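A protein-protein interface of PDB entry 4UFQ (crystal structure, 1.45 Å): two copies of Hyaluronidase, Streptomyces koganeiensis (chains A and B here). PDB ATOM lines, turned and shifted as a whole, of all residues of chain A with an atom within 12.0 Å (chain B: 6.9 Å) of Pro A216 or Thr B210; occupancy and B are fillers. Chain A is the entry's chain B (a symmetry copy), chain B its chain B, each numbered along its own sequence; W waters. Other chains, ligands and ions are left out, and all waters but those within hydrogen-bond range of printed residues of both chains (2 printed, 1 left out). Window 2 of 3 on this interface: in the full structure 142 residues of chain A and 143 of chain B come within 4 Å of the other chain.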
ATOM      1  N   VAL A 175     -22.896  16.224 -36.381  1.00  0.00           N
ATOM      2  CA  VAL A 175     -21.553  16.319 -35.827  1.00  0.00           C
ATOM      3  C   VAL A 175     -21.589  15.823 -34.401  1.00  0.00           C
ATOM      4  O   VAL A 175     -22.221  16.454 -33.528  1.00  0.00           O
ATOM      5  CB  VAL A 175     -21.023  17.763 -35.804  1.00  0.00           C
ATOM      6  CG1 VAL A 175     -19.599  17.830 -35.184  1.00  0.00           C
ATOM      7  CG2 VAL A 175     -21.041  18.359 -37.205  1.00  0.00           C
ATOM      8  N   ILE A 177     -19.677  15.250 -30.893  1.00  0.00           N
ATOM      9  CA  ILE A 177     -18.554  15.777 -30.143  1.00  0.00           C
ATOM     10  C   ILE A 177     -18.488  14.991 -28.849  1.00  0.00           C
ATOM     11  O   ILE A 177     -19.417  15.063 -28.030  1.00  0.00           O
ATOM     12  CB  ILE A 177     -18.725  17.279 -29.855  1.00  0.00           C
ATOM     13  CG1 ILE A 177     -18.879  18.060 -31.167  1.00  0.00           C
ATOM     14  CG2 ILE A 177     -17.526  17.791 -29.045  1.00  0.00           C
ATOM     15  CD1 ILE A 177     -19.236  19.528 -30.968  1.00  0.00           C
ATOM     16  N   ASN A 179     -17.019  13.900 -25.034  1.00  0.00           N
ATOM     17  CA  ASN A 179     -16.586  14.734 -23.910  1.00  0.00           C
ATOM     18  C   ASN A 179     -15.081  14.991 -23.999  1.00  0.00           C
ATOM     19  O   ASN A 179     -14.292  14.072 -24.252  1.00  0.00           O
ATOM     20  CB  ASN A 179     -16.872  14.076 -22.570  1.00  0.00           C
ATOM     21  CG  ASN A 179     -18.369  14.001 -22.213  1.00  0.00           C
ATOM     22  OD1 ASN A 179     -19.141  14.929 -22.478  1.00  0.00           O
ATOM     23  ND2 ASN A 179     -18.768  12.879 -21.637  1.00  0.00           N
ATOM     24  N   LEU A 195     -15.253  25.146 -28.747  1.00  0.00           N
ATOM     25  CA  LEU A 195     -16.519  24.460 -28.572  1.00  0.00           C
ATOM     26  C   LEU A 195     -16.183  23.071 -28.081  1.00  0.00           C
ATOM     27  O   LEU A 195     -15.313  22.399 -28.659  1.00  0.00           O
ATOM     28  CB  LEU A 195     -17.251  24.377 -29.915  1.00  0.00           C
ATOM     29  CG  LEU A 195     -18.665  23.794 -29.923  1.00  0.00           C
ATOM     30  CD1 LEU A 195     -19.664  24.704 -29.197  1.00  0.00           C
ATOM     31  CD2 LEU A 195     -19.137  23.535 -31.356  1.00  0.00           C
ATOM     32  N   TYR A 196     -16.783  22.627 -26.982  1.00  0.00           N
ATOM     33  CA  TYR A 196     -16.472  21.310 -26.451  1.00  0.00           C
ATOM     34  C   TYR A 196     -17.631  20.745 -25.694  1.00  0.00           C
ATOM     35  O   TYR A 196     -18.537  21.484 -25.286  1.00  0.00           O
ATOM     36  CB  TYR A 196     -15.214  21.356 -25.557  1.00  0.00           C
ATOM     37  CG  TYR A 196     -15.301  22.247 -24.333  1.00  0.00           C
ATOM     38  CD1 TYR A 196     -15.150  23.628 -24.445  1.00  0.00           C
ATOM     39  CD2 TYR A 196     -15.530  21.716 -23.091  1.00  0.00           C
ATOM     40  CE1 TYR A 196     -15.205  24.455 -23.319  1.00  0.00           C
ATOM     41  CE2 TYR A 196     -15.585  22.529 -21.961  1.00  0.00           C
ATOM     42  CZ  TYR A 196     -15.435  23.896 -22.093  1.00  0.00           C
ATOM     43  OH  TYR A 196     -15.490  24.708 -20.989  1.00  0.00           O
ATOM     44  N   ALA A 197     -17.620  19.427 -25.529  1.00  0.00           N
ATOM     45  CA  ALA A 197     -18.579  18.746 -24.681  1.00  0.00           C
ATOM     46  C   ALA A 197     -17.969  18.434 -23.320  1.00  0.00           C
ATOM     47  O   ALA A 197     -16.778  18.139 -23.195  1.00  0.00           O
ATOM     48  CB  ALA A 197     -19.123  17.458 -25.362  1.00  0.00           C
ATOM     49  N   SER A 198     -18.811  18.554 -22.294  1.00  0.00           N
ATOM     50  CA  SER A 198     -18.392  18.333 -20.925  1.00  0.00           C
ATOM     51  C   SER A 198     -19.588  17.754 -20.177  1.00  0.00           C
ATOM     52  O   SER A 198     -20.649  18.389 -20.091  1.00  0.00           O
ATOM     53  CB  SER A 198     -17.938  19.649 -20.329  1.00  0.00           C
ATOM     54  OG  SER A 198     -17.316  19.412 -19.068  1.00  0.00           O
ATOM     55  N   GLY A 199     -19.435  16.541 -19.662  1.00  0.00           N
ATOM     56  CA  GLY A 199     -20.513  15.868 -18.957  1.00  0.00           C
ATOM     57  C   GLY A 199     -21.757  15.718 -19.810  1.00  0.00           C
ATOM     58  O   GLY A 199     -22.855  15.700 -19.262  1.00  0.00           O
ATOM     59  N   GLY A 200     -21.606  15.619 -21.127  1.00  0.00           N
ATOM     60  CA  GLY A 200     -22.737  15.459 -22.039  1.00  0.00           C
ATOM     61  C   GLY A 200     -23.367  16.763 -22.514  1.00  0.00           C
ATOM     62  O   GLY A 200     -24.224  16.758 -23.390  1.00  0.00           O
ATOM     63  N   ALA A 201     -22.949  17.881 -21.926  1.00  0.00           N
ATOM     64  CA  ALA A 201     -23.435  19.225 -22.279  1.00  0.00           C
ATOM     65  C   ALA A 201     -22.521  19.848 -23.326  1.00  0.00           C
ATOM     66  O   ALA A 201     -21.358  19.430 -23.468  1.00  0.00           O
ATOM     67  CB  ALA A 201     -23.472  20.089 -21.041  1.00  0.00           C
ATOM     68  N   LEU A 202     -23.025  20.849 -24.045  1.00  0.00           N
ATOM     69  CA  LEU A 202     -22.255  21.581 -25.041  1.00  0.00           C
ATOM     70  C   LEU A 202     -21.869  22.944 -24.465  1.00  0.00           C
ATOM     71  O   LEU A 202     -22.739  23.676 -23.948  1.00  0.00           O
ATOM     72  CB  LEU A 202     -23.094  21.744 -26.320  1.00  0.00           C
ATOM     73  CG  LEU A 202     -22.374  22.428 -27.483  1.00  0.00           C
ATOM     74  CD1 LEU A 202     -21.238  21.565 -28.026  1.00  0.00           C
ATOM     75  CD2 LEU A 202     -23.409  22.755 -28.583  1.00  0.00           C
ATOM     76  N   LEU A 203     -20.573  23.273 -24.523  1.00  0.00           N
ATOM     77  CA  LEU A 203     -20.020  24.489 -23.924  1.00  0.00           C
ATOM     78  C   LEU A 203     -19.216  25.281 -24.933  1.00  0.00           C
ATOM     79  O   LEU A 203     -18.647  24.696 -25.861  1.00  0.00           O
ATOM     80  CB  LEU A 203     -19.111  24.150 -22.733  1.00  0.00           C
ATOM     81  CG  LEU A 203     -19.769  23.778 -21.396  1.00  0.00           C
ATOM     82  CD1 LEU A 203     -20.479  22.461 -21.455  1.00  0.00           C
ATOM     83  CD2 LEU A 203     -18.752  23.766 -20.251  1.00  0.00           C
ATOM     84  N   TRP A 204     -19.121  26.594 -24.740  1.00  0.00           N
ATOM     85  CA  TRP A 204     -18.225  27.466 -25.504  1.00  0.00           C
ATOM     86  C   TRP A 204     -17.396  28.292 -24.556  1.00  0.00           C
ATOM     87  O   TRP A 204     -17.921  28.940 -23.633  1.00  0.00           O
ATOM     88  CB  TRP A 204     -19.023  28.452 -26.352  1.00  0.00           C
ATOM     89  CG  TRP A 204     -18.271  29.530 -27.141  1.00  0.00           C
ATOM     90  CD1 TRP A 204     -18.221  30.868 -26.863  1.00  0.00           C
ATOM     91  CD2 TRP A 204     -17.582  29.358 -28.389  1.00  0.00           C
ATOM     92  NE1 TRP A 204     -17.538  31.527 -27.843  1.00  0.00           N
ATOM     93  CE2 TRP A 204     -17.131  30.625 -28.794  1.00  0.00           C
ATOM     94  CE3 TRP A 204     -17.284  28.253 -29.183  1.00  0.00           C
ATOM     95  CZ2 TRP A 204     -16.436  30.822 -29.982  1.00  0.00           C
ATOM     96  CZ3 TRP A 204     -16.591  28.450 -30.353  1.00  0.00           C
ATOM     97  CH2 TRP A 204     -16.149  29.714 -30.726  1.00  0.00           C
ATOM     98  N   THR A 212     -19.654  29.355 -21.309  1.00  0.00           N
ATOM     99  CA  THR A 212     -21.114  29.249 -21.342  1.00  0.00           C
ATOM    100  C   THR A 212     -21.541  27.825 -21.632  1.00  0.00           C
ATOM    101  O   THR A 212     -21.033  27.207 -22.562  1.00  0.00           O
ATOM    102  CB  THR A 212     -21.665  30.130 -22.455  1.00  0.00           C
ATOM    103  OG1 THR A 212     -21.280  31.485 -22.220  1.00  0.00           O
ATOM    104  CG2 THR A 212     -23.190  30.074 -22.523  1.00  0.00           C
ATOM    105  N   THR A 213     -22.457  27.273 -20.827  1.00  0.00           N
ATOM    106  CA  THR A 213     -23.102  25.999 -21.154  1.00  0.00           C
ATOM    107  C   THR A 213     -24.283  26.312 -22.077  1.00  0.00           C
ATOM    108  O   THR A 213     -25.296  26.901 -21.643  1.00  0.00           O
ATOM    109  CB  THR A 213     -23.551  25.256 -19.888  1.00  0.00           C
ATOM    110  OG1 THR A 213     -22.427  25.007 -19.035  1.00  0.00           O
ATOM    111  CG2 THR A 213     -24.164  23.914 -20.251  1.00  0.00           C
ATOM    112  N   ILE A 214     -24.123  25.959 -23.344  1.00  0.00           N
ATOM    113  CA  ILE A 214     -25.117  26.241 -24.365  1.00  0.00           C
ATOM    114  C   ILE A 214     -26.313  25.306 -24.300  1.00  0.00           C
ATOM    115  O   ILE A 214     -27.451  25.755 -24.472  1.00  0.00           O
ATOM    116  CB  ILE A 214     -24.460  26.131 -25.760  1.00  0.00           C
ATOM    117  CG1 ILE A 214     -23.389  27.212 -25.893  1.00  0.00           C
ATOM    118  CG2 ILE A 214     -25.502  26.219 -26.864  1.00  0.00           C
ATOM    119  CD1 ILE A 214     -22.437  26.934 -27.056  1.00  0.00           C
ATOM    120  N   ALA A 215     -26.076  24.017 -24.036  1.00  0.00           N
ATOM    121  CA  ALA A 215     -27.182  23.064 -23.996  1.00  0.00           C
ATOM    122  C   ALA A 215     -26.841  21.940 -23.061  1.00  0.00           C
ATOM    123  O   ALA A 215     -25.701  21.502 -23.012  1.00  0.00           O
ATOM    124  CB  ALA A 215     -27.489  22.516 -25.366  1.00  0.00           C
ATOM    125  N   PRO A 216     -27.838  21.420 -22.340  1.00  0.00           N
ATOM    126  CA  PRO A 216     -27.550  20.386 -21.333  1.00  0.00           C
ATOM    127  C   PRO A 216     -27.403  18.971 -21.883  1.00  0.00           C
ATOM    128  O   PRO A 216     -27.815  18.655 -23.001  1.00  0.00           O
ATOM    129  CB  PRO A 216     -28.774  20.451 -20.414  1.00  0.00           C
ATOM    130  CG  PRO A 216     -29.877  20.943 -21.290  1.00  0.00           C
ATOM    131  CD  PRO A 216     -29.227  21.889 -22.272  1.00  0.00           C
ATOM    132  N   ALA A 217     -26.806  18.106 -21.079  1.00  0.00           N
ATOM    133  CA  ALA A 217     -26.825  16.684 -21.353  1.00  0.00           C
ATOM    134  C   ALA A 217     -28.259  16.182 -21.392  1.00  0.00           C
ATOM    135  O   ALA A 217     -28.564  15.269 -22.162  1.00  0.00           O
ATOM    136  CB  ALA A 217     -26.055  15.940 -20.285  1.00  0.00           C
ATOM    137  OXT ALA A 217     -29.132  16.674 -20.654  1.00  0.00           O
ATOM    138  N   TRP B 204     -28.889  20.445 -30.238  1.00  0.00           N
ATOM    139  CA  TRP B 204     -27.974  19.522 -29.561  1.00  0.00           C
ATOM    140  C   TRP B 204     -28.768  18.463 -28.842  1.00  0.00           C
ATOM    141  O   TRP B 204     -29.701  18.763 -28.076  1.00  0.00           O
ATOM    142  CB  TRP B 204     -27.161  20.252 -28.497  1.00  0.00           C
ATOM    143  CG  TRP B 204     -26.225  19.441 -27.594  1.00  0.00           C
ATOM    144  CD1 TRP B 204     -26.409  19.146 -26.272  1.00  0.00           C
ATOM    145  CD2 TRP B 204     -24.919  18.947 -27.933  1.00  0.00           C
ATOM    146  NE1 TRP B 204     -25.317  18.493 -25.779  1.00  0.00           N
ATOM    147  CE2 TRP B 204     -24.386  18.353 -26.778  1.00  0.00           C
ATOM    148  CE3 TRP B 204     -24.169  18.927 -29.106  1.00  0.00           C
ATOM    149  CZ2 TRP B 204     -23.115  17.787 -26.751  1.00  0.00           C
ATOM    150  CZ3 TRP B 204     -22.918  18.359 -29.079  1.00  0.00           C
ATOM    151  CH2 TRP B 204     -22.417  17.773 -27.924  1.00  0.00           C
ATOM    152  N   ARG B 205     -28.397  17.210 -29.081  1.00  0.00           N
ATOM    153  CA  ARG B 205     -28.818  16.082 -28.271  1.00  0.00           C
ATOM    154  C   ARG B 205     -27.683  15.726 -27.320  1.00  0.00           C
ATOM    155  O   ARG B 205     -26.589  15.388 -27.776  1.00  0.00           O
ATOM    156  CB  ARG B 205     -29.188  14.886 -29.145  1.00  0.00           C
ATOM    157  CG  ARG B 205     -29.321  13.576 -28.352  1.00  0.00           C
ATOM    158  CD  ARG B 205     -29.728  12.396 -29.214  1.00  0.00           C
ATOM    159  NE  ARG B 205     -31.172  12.358 -29.342  1.00  0.00           N
ATOM    160  CZ  ARG B 205     -31.998  11.740 -28.507  1.00  0.00           C
ATOM    161  NH1 ARG B 205     -31.546  11.075 -27.458  1.00  0.00           N
ATOM    162  NH2 ARG B 205     -33.308  11.803 -28.717  1.00  0.00           N
ATOM    163  N   GLY B 206     -27.913  15.828 -26.022  1.00  0.00           N
ATOM    164  CA  GLY B 206     -26.911  15.467 -25.038  1.00  0.00           C
ATOM    165  C   GLY B 206     -26.923  14.003 -24.663  1.00  0.00           C
ATOM    166  O   GLY B 206     -27.844  13.233 -25.008  1.00  0.00           O
ATOM    167  N   SER B 207     -25.951  13.605 -23.854  1.00  0.00           N
ATOM    168  CA  SER B 207     -25.778  12.184 -23.556  1.00  0.00           C
ATOM    169  C   SER B 207     -26.902  11.613 -22.720  1.00  0.00           C
ATOM    170  O   SER B 207     -27.087  10.396 -22.705  1.00  0.00           O
ATOM    171  CB  SER B 207     -24.435  11.913 -22.883  1.00  0.00           C
ATOM    172  OG  SER B 207     -24.324  12.602 -21.662  1.00  0.00           O
ATOM    173  N   ASN B 208     -27.627  12.465 -22.000  1.00  0.00           N
ATOM    174  CA  ASN B 208     -28.737  11.995 -21.187  1.00  0.00           C
ATOM    175  C   ASN B 208     -30.045  12.041 -21.968  1.00  0.00           C
ATOM    176  O   ASN B 208     -31.102  11.683 -21.446  1.00  0.00           O
ATOM    177  CB  ASN B 208     -28.868  12.791 -19.883  1.00  0.00           C
ATOM    178  CG  ASN B 208     -27.810  12.415 -18.863  1.00  0.00           C
ATOM    179  OD1 ASN B 208     -27.279  11.299 -18.882  1.00  0.00           O
ATOM    180  ND2 ASN B 208     -27.503  13.344 -17.961  1.00  0.00           N
ATOM    181  N   GLY B 209     -29.955  12.437 -23.230  1.00  0.00           N
ATOM    182  CA  GLY B 209     -31.091  12.400 -24.131  1.00  0.00           C
ATOM    183  C   GLY B 209     -31.853  13.705 -24.244  1.00  0.00           C
ATOM    184  O   GLY B 209     -32.883  13.765 -24.902  1.00  0.00           O
ATOM    185  N   THR B 210     -31.365  14.768 -23.616  1.00  0.00           N
ATOM    186  CA  THR B 210     -32.053  16.056 -23.737  1.00  0.00           C
ATOM    187  C   THR B 210     -31.794  16.666 -25.082  1.00  0.00           C
ATOM    188  O   THR B 210     -30.635  16.732 -25.519  1.00  0.00           O
ATOM    189  CB  THR B 210     -31.604  17.042 -22.658  1.00  0.00           C
ATOM    190  OG1 THR B 210     -31.662  16.398 -21.379  1.00  0.00           O
ATOM    191  CG2 THR B 210     -32.479  18.309 -22.665  1.00  0.00           C
ATOM    192  N   VAL B 211     -32.849  17.126 -25.751  1.00  0.00           N
ATOM    193  CA  VAL B 211     -32.736  17.767 -27.059  1.00  0.00           C
ATOM    194  C   VAL B 211     -33.102  19.238 -26.918  1.00  0.00           C
ATOM    195  O   VAL B 211     -34.197  19.562 -26.452  1.00  0.00           O
ATOM    196  CB  VAL B 211     -33.615  17.051 -28.098  1.00  0.00           C
ATOM    197  CG1 VAL B 211     -33.428  17.682 -29.446  1.00  0.00           C
ATOM    198  CG2 VAL B 211     -33.237  15.562 -28.167  1.00  0.00           C
ATOM    199  N   THR B 212     -32.175  20.109 -27.276  1.00  0.00           N
ATOM    200  CA  THR B 212     -32.315  21.560 -27.142  1.00  0.00           C
ATOM    201  C   THR B 212     -32.167  22.240 -28.487  1.00  0.00           C
ATOM    202  O   THR B 212     -31.227  21.954 -29.221  1.00  0.00           O
ATOM    203  CB  THR B 212     -31.217  22.097 -26.233  1.00  0.00           C
ATOM    204  OG1 THR B 212     -31.319  21.477 -24.950  1.00  0.00           O
ATOM    205  CG2 THR B 212     -31.327  23.609 -26.039  1.00  0.00           C
HETATM  206  O   HOH W   1     -24.026  13.357 -18.108  1.00  0.00           O
HETATM  207  O   HOH W   2     -21.501  12.129 -21.682  1.00  0.00           O
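The chain-end carboxylate (O) of Ala A217 is in hydrogen-bond range of the backbone NH (N) of Asn B208 (3.0 Å). The indole nitrogen of Trp B204 sits at hydrogen-bond distance from the backbone carbonyl oxygen of Gly A200 (3.1 Å). OG1 of Thr B210 lies within hydrogen-bond range of OXT of Ala A217 (2.6 Å). N of Gly B209 is in hydrogen-bond range of O of Ala A217, at 3.3 Å.
The backbone carbonyl oxygen of Trp B204 is in hydrogen-bond range of the backbone NH of Thr B212, 2.9 Å away. N of Leu A202 is in hydrogen-bond range of O of Ala A215, 2.9 Å away. The side-chain amide oxygen of Asn A179 is in hydrogen-bond range of the backbone NH of Gly A200 (2.9 Å). N of Ile A214 is in hydrogen-bond range of O of Leu A202 (2.7 Å).
Among the printed residues, pairs that only touch across the chains: Gly A200 with Gly B206, Gly A200 with Ser B207, Ala A201 with Trp B204, Leu A202 with Trp B204, Ala A215 with Trp B204, Ala A215 with Thr B212, Pro A216 with Trp B204, Pro A216 with Gly B206, Pro A216 with Thr B210, Pro A216 with Thr B212, Ala A217 with Gly B206 and Ala A217 with Ser B207.
Pro A216 touches four residues of chain B. Trp B204 touches just these residues of chain A: Gly A200 (3.1 Å), Ala A201 (3.96 Å), Leu A202 (3.7 Å), Ala A215 (3.7 Å) and Pro A216 (3.6 Å). Arg B205 touches none of the printed residues of chain A. Ser B207 touches just these residues of chain A: Gly A200 and Ala A217. Asn B208 touches one residue of chain A. Of chain A, only Ala A217 comes within 4 Å of Gly B209. Val B211 touches none of the printed residues of chain A. Of the printed residues of chain B, Gly A200 touches Trp B204, Gly B206 and Ser B207. Printed residues of chain B within 4 Å of Leu A202: Trp B204 (3.7 Å). Printed residues of chain B within 4 Å of Ala A215: Trp B204 and Thr B212. Ile A214 touches none of the printed residues of chain B. Trp A204 touches none of the printed residues of chain B. The nearest residue of chain A that does not touch Thr B210 is Ala A215 (6.6 Å). The nearest printed residue of chain B that does not touch Ala A215 is Gly B206 (6.5 Å).
Of the 19 printed residues of chain A, 6 touch a printed residue of chain B. Printed residues of chain A that touch a printed residue of chain B: Gly A200, Ala A201, Leu A202, Ala A215, Pro A216 and Ala A217. Hydrophobic or aromatic side chains of chain A within 4 Å of the printed part of chain B: Leu A202, Ala A215, Pro A216 and Ala A217. Among the printed residues, 16 pairs touch across the chains.
2 positions are printed for both chains.
Water W2 bridges ND2 of Asn A179 (2.8 Å) and OG of Ser B207 (2.9 Å). Water W1 lies within hydrogen-bond range of O of Gly A199 (2.9 Å) and ND2 of Asn B208 (3.5 Å).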
